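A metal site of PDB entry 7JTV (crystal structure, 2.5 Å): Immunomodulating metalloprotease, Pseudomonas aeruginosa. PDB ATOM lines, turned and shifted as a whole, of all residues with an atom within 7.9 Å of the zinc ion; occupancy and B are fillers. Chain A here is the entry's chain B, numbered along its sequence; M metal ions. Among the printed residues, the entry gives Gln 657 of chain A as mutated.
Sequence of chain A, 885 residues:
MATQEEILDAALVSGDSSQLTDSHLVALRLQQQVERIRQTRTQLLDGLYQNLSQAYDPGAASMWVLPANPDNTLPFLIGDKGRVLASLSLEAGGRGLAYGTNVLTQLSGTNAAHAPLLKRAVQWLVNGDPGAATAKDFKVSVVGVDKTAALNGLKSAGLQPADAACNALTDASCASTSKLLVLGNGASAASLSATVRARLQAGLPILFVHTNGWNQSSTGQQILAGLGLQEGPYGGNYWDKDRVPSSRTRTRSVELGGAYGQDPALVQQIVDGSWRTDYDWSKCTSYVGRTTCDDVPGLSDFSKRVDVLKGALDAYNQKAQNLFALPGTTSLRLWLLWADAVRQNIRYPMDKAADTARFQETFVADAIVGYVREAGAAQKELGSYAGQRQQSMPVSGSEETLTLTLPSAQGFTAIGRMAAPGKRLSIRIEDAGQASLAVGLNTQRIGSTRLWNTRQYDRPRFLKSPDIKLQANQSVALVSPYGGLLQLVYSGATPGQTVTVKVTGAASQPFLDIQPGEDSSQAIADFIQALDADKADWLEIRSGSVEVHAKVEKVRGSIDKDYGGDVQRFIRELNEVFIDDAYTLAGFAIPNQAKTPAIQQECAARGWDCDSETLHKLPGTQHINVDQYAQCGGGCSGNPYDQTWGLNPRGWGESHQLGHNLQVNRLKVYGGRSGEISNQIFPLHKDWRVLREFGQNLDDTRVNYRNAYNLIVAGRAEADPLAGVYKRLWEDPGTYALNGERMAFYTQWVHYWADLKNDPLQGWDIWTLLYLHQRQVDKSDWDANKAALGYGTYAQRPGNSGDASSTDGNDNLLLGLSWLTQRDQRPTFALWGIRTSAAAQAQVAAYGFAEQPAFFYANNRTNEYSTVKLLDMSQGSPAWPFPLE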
ATOM      1  N   GLY A 635      15.052  24.946  -9.219  1.00  0.00           N
ATOM      2  CA  GLY A 635      15.922  25.424  -8.170  1.00  0.00           C
ATOM      3  C   GLY A 635      17.330  24.917  -8.415  1.00  0.00           C
ATOM      4  O   GLY A 635      17.521  23.733  -8.705  1.00  0.00           O
ATOM      5  N   CYS A 636      18.336  25.783  -8.293  1.00  0.00           N
ATOM      6  CA  CYS A 636      19.709  25.431  -8.608  1.00  0.00           C
ATOM      7  C   CYS A 636      20.619  25.823  -7.456  1.00  0.00           C
ATOM      8  O   CYS A 636      20.466  26.900  -6.876  1.00  0.00           O
ATOM      9  CB  CYS A 636      20.199  26.108  -9.904  1.00  0.00           C
ATOM     10  SG  CYS A 636      21.419  25.160 -10.836  1.00  0.00           S
ATOM     11  N   SER A 637      21.565  24.948  -7.143  1.00  0.00           N
ATOM     12  CA  SER A 637      22.500  25.143  -6.058  1.00  0.00           C
ATOM     13  C   SER A 637      23.519  26.232  -6.398  1.00  0.00           C
ATOM     14  O   SER A 637      23.753  26.542  -7.567  1.00  0.00           O
ATOM     15  CB  SER A 637      23.242  23.845  -5.773  1.00  0.00           C
ATOM     16  OG  SER A 637      23.578  23.215  -7.003  1.00  0.00           O
ATOM     17  N   TRP A 652      11.509  22.285   2.701  1.00  0.00           N
ATOM     18  CA  TRP A 652      12.626  21.366   2.588  1.00  0.00           C
ATOM     19  C   TRP A 652      13.717  21.912   1.661  1.00  0.00           C
ATOM     20  O   TRP A 652      14.912  21.846   1.979  1.00  0.00           O
ATOM     21  CB  TRP A 652      12.125  20.014   2.094  1.00  0.00           C
ATOM     22  CG  TRP A 652      13.221  19.041   1.853  1.00  0.00           C
ATOM     23  CD1 TRP A 652      14.030  18.973   0.749  1.00  0.00           C
ATOM     24  CD2 TRP A 652      13.658  18.004   2.748  1.00  0.00           C
ATOM     25  NE1 TRP A 652      14.936  17.942   0.900  1.00  0.00           N
ATOM     26  CE2 TRP A 652      14.728  17.333   2.105  1.00  0.00           C
ATOM     27  CE3 TRP A 652      13.231  17.567   4.008  1.00  0.00           C
ATOM     28  CZ2 TRP A 652      15.394  16.237   2.706  1.00  0.00           C
ATOM     29  CZ3 TRP A 652      13.899  16.479   4.597  1.00  0.00           C
ATOM     30  CH2 TRP A 652      14.969  15.826   3.941  1.00  0.00           C
ATOM     31  N   GLY A 653      13.315  22.407   0.488  1.00  0.00           N
ATOM     32  CA  GLY A 653      14.305  22.902  -0.456  1.00  0.00           C
ATOM     33  C   GLY A 653      15.131  24.047   0.082  1.00  0.00           C
ATOM     34  O   GLY A 653      16.315  24.185  -0.272  1.00  0.00           O
ATOM     35  N   HIS A 656      17.810  22.261   2.314  1.00  0.00           N
ATOM     36  CA  HIS A 656      18.671  21.447   1.456  1.00  0.00           C
ATOM     37  C   HIS A 656      19.743  22.297   0.796  1.00  0.00           C
ATOM     38  O   HIS A 656      20.945  22.022   0.913  1.00  0.00           O
ATOM     39  CB  HIS A 656      17.834  20.703   0.397  1.00  0.00           C
ATOM     40  CG  HIS A 656      18.642  19.845  -0.527  1.00  0.00           C
ATOM     41  ND1 HIS A 656      18.833  18.504  -0.308  1.00  0.00           N
ATOM     42  CD2 HIS A 656      19.296  20.135  -1.680  1.00  0.00           C
ATOM     43  CE1 HIS A 656      19.582  17.999  -1.278  1.00  0.00           C
ATOM     44  NE2 HIS A 656      19.868  18.969  -2.125  1.00  0.00           N
ATOM     45  N   GLN A 657      19.329  23.378   0.128  1.00  0.00           N
ATOM     46  CA  GLN A 657      20.268  24.196  -0.629  1.00  0.00           C
ATOM     47  C   GLN A 657      21.241  24.920   0.289  1.00  0.00           C
ATOM     48  O   GLN A 657      22.440  24.983   0.007  1.00  0.00           O
ATOM     49  CB  GLN A 657      19.527  25.210  -1.502  1.00  0.00           C
ATOM     50  CG  GLN A 657      18.778  24.594  -2.657  1.00  0.00           C
ATOM     51  CD  GLN A 657      19.664  24.131  -3.777  1.00  0.00           C
ATOM     52  OE1 GLN A 657      20.847  23.838  -3.589  1.00  0.00           O
ATOM     53  NE2 GLN A 657      19.089  24.056  -4.965  1.00  0.00           N
ATOM     54  N   HIS A 660      23.974  22.656   1.250  1.00  0.00           N
ATOM     55  CA  HIS A 660      25.060  22.370   0.314  1.00  0.00           C
ATOM     56  C   HIS A 660      26.247  23.312   0.554  1.00  0.00           C
ATOM     57  O   HIS A 660      27.403  22.864   0.574  1.00  0.00           O
ATOM     58  CB  HIS A 660      24.572  22.478  -1.140  1.00  0.00           C
ATOM     59  CG  HIS A 660      23.959  21.230  -1.692  1.00  0.00           C
ATOM     60  ND1 HIS A 660      24.511  19.970  -1.516  1.00  0.00           N
ATOM     61  CD2 HIS A 660      22.846  21.047  -2.446  1.00  0.00           C
ATOM     62  CE1 HIS A 660      23.759  19.078  -2.132  1.00  0.00           C
ATOM     63  NE2 HIS A 660      22.741  19.699  -2.700  1.00  0.00           N
ATOM     64  N   GLN A 663      28.407  22.080   3.477  1.00  0.00           N
ATOM     65  CA  GLN A 663      29.004  20.755   3.465  1.00  0.00           C
ATOM     66  C   GLN A 663      30.502  20.865   3.650  1.00  0.00           C
ATOM     67  O   GLN A 663      31.109  21.869   3.281  1.00  0.00           O
ATOM     68  CB  GLN A 663      28.684  20.015   2.175  1.00  0.00           C
ATOM     69  CG  GLN A 663      27.361  19.230   2.237  1.00  0.00           C
ATOM     70  CD  GLN A 663      26.876  18.798   0.870  1.00  0.00           C
ATOM     71  OE1 GLN A 663      26.590  17.633   0.639  1.00  0.00           O
ATOM     72  NE2 GLN A 663      26.806  19.744  -0.061  1.00  0.00           N
ATOM     73  N   GLY A 675      27.195  13.389  -1.573  1.00  0.00           N
ATOM     74  CA  GLY A 675      27.056  14.757  -2.036  1.00  0.00           C
ATOM     75  C   GLY A 675      25.655  15.335  -1.897  1.00  0.00           C
ATOM     76  O   GLY A 675      25.498  16.539  -1.727  1.00  0.00           O
ATOM     77  N   GLU A 676      24.628  14.481  -1.996  1.00  0.00           N
ATOM     78  CA  GLU A 676      23.250  14.865  -1.721  1.00  0.00           C
ATOM     79  C   GLU A 676      22.721  14.182  -0.470  1.00  0.00           C
ATOM     80  O   GLU A 676      21.515  13.941  -0.333  1.00  0.00           O
ATOM     81  CB  GLU A 676      22.364  14.537  -2.928  1.00  0.00           C
ATOM     82  CG  GLU A 676      22.763  15.289  -4.195  1.00  0.00           C
ATOM     83  CD  GLU A 676      22.278  16.729  -4.214  1.00  0.00           C
ATOM     84  OE1 GLU A 676      21.422  17.093  -3.379  1.00  0.00           O
ATOM     85  OE2 GLU A 676      22.756  17.499  -5.077  1.00  0.00           O
ATOM     86  N   ILE A 677      23.611  13.852   0.478  1.00  0.00           N
ATOM     87  CA  ILE A 677      23.233  13.166   1.698  1.00  0.00           C
ATOM     88  C   ILE A 677      23.667  13.945   2.938  1.00  0.00           C
ATOM     89  O   ILE A 677      22.876  14.133   3.868  1.00  0.00           O
ATOM     90  CB  ILE A 677      23.803  11.736   1.747  1.00  0.00           C
ATOM     91  CG1 ILE A 677      23.414  10.970   0.490  1.00  0.00           C
ATOM     92  CG2 ILE A 677      23.321  11.039   2.996  1.00  0.00           C
ATOM     93  CD1 ILE A 677      21.949  10.580   0.469  1.00  0.00           C
ATOM     94  N   ASN A 679      24.453  17.124   3.417  1.00  0.00           N
ATOM     95  CA  ASN A 679      23.716  18.371   3.649  1.00  0.00           C
ATOM     96  C   ASN A 679      22.289  18.137   4.123  1.00  0.00           C
ATOM     97  O   ASN A 679      21.618  19.102   4.488  1.00  0.00           O
ATOM     98  CB  ASN A 679      23.684  19.208   2.384  1.00  0.00           C
ATOM     99  CG  ASN A 679      22.867  18.540   1.277  1.00  0.00           C
ATOM    100  OD1 ASN A 679      22.885  17.304   1.158  1.00  0.00           O
ATOM    101  ND2 ASN A 679      22.149  19.338   0.490  1.00  0.00           N
ATOM    102  N   GLN A 680      21.794  16.889   4.099  1.00  0.00           N
ATOM    103  CA  GLN A 680      20.400  16.668   4.465  1.00  0.00           C
ATOM    104  C   GLN A 680      20.135  16.775   5.955  1.00  0.00           C
ATOM    105  O   GLN A 680      18.974  16.857   6.347  1.00  0.00           O
ATOM    106  CB  GLN A 680      19.908  15.303   3.954  1.00  0.00           C
ATOM    107  CG  GLN A 680      20.028  15.180   2.457  1.00  0.00           C
ATOM    108  CD  GLN A 680      18.798  15.705   1.752  1.00  0.00           C
ATOM    109  OE1 GLN A 680      18.516  16.906   1.812  1.00  0.00           O
ATOM    110  NE2 GLN A 680      18.060  14.825   1.084  1.00  0.00           N
ATOM    111  N   THR A 735      23.753  10.373  -9.044  1.00  0.00           N
ATOM    112  CA  THR A 735      23.871  11.547  -8.176  1.00  0.00           C
ATOM    113  C   THR A 735      22.753  11.644  -7.136  1.00  0.00           C
ATOM    114  O   THR A 735      22.917  12.365  -6.147  1.00  0.00           O
ATOM    115  CB  THR A 735      23.921  12.847  -9.001  1.00  0.00           C
ATOM    116  OG1 THR A 735      23.026  12.769 -10.101  1.00  0.00           O
ATOM    117  CG2 THR A 735      25.347  13.102  -9.522  1.00  0.00           C
ATOM    118  N   TYR A 736      21.631  10.933  -7.314  1.00  0.00           N
ATOM    119  CA  TYR A 736      20.642  10.851  -6.241  1.00  0.00           C
ATOM    120  C   TYR A 736      20.339   9.419  -5.832  1.00  0.00           C
ATOM    121  O   TYR A 736      19.297   9.153  -5.223  1.00  0.00           O
ATOM    122  CB  TYR A 736      19.346  11.570  -6.624  1.00  0.00           C
ATOM    123  CG  TYR A 736      19.550  12.973  -7.140  1.00  0.00           C
ATOM    124  CD1 TYR A 736      19.428  14.085  -6.285  1.00  0.00           C
ATOM    125  CD2 TYR A 736      19.869  13.208  -8.482  1.00  0.00           C
ATOM    126  CE1 TYR A 736      19.621  15.399  -6.769  1.00  0.00           C
ATOM    127  CE2 TYR A 736      20.069  14.502  -8.971  1.00  0.00           C
ATOM    128  CZ  TYR A 736      19.941  15.592  -8.115  1.00  0.00           C
ATOM    129  OH  TYR A 736      20.127  16.870  -8.617  1.00  0.00           O
ATOM    130  N   ASN A 739      19.195   7.710  -1.994  1.00  0.00           N
ATOM    131  CA  ASN A 739      19.300   8.943  -1.227  1.00  0.00           C
ATOM    132  C   ASN A 739      18.651   8.827   0.148  1.00  0.00           C
ATOM    133  O   ASN A 739      19.228   9.236   1.154  1.00  0.00           O
ATOM    134  CB  ASN A 739      18.679  10.108  -2.016  1.00  0.00           C
ATOM    135  CG  ASN A 739      18.688  11.420  -1.243  1.00  0.00           C
ATOM    136  OD1 ASN A 739      17.816  11.686  -0.419  1.00  0.00           O
ATOM    137  ND2 ASN A 739      19.706  12.239  -1.486  1.00  0.00           N
HETATM  138 ZN    ZN M   1      20.949  19.053  -3.875  1.00  0.00          ZN
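O of His 656 is in hydrogen-bond range of ND2 of Asn 679 (3.0 Å). ND1 of His 656 lies within hydrogen-bond range of OE1 of Gln 680 (2.7 Å). The backbone carbonyl oxygen of Glu 676 lies within hydrogen-bond range of the side-chain amide nitrogen of Asn 739 (2.7 Å). A ring nitrogen (ND1) of His 660 sits close to the side-chain amide nitrogen of Asn 679, at 3.2 Å. A ring nitrogen (ND1) of His 660 is in hydrogen-bond range of the side-chain amide nitrogen of Gln 663 (2.7 Å).
Within 4 Å of the zinc ion: His 656, His 660 and Glu 676. The nearest printed residue that does not touch the zinc ion is Asn 679 (4.5 Å).
The zinc ion is bound by NE2 of His 656, OE1 of Glu 676 and NE2 of His 660. The zinc ion has three donor atoms within binding distance. Slightly farther from the zinc ion lies OE2 of Glu 676 (2.7 Å).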
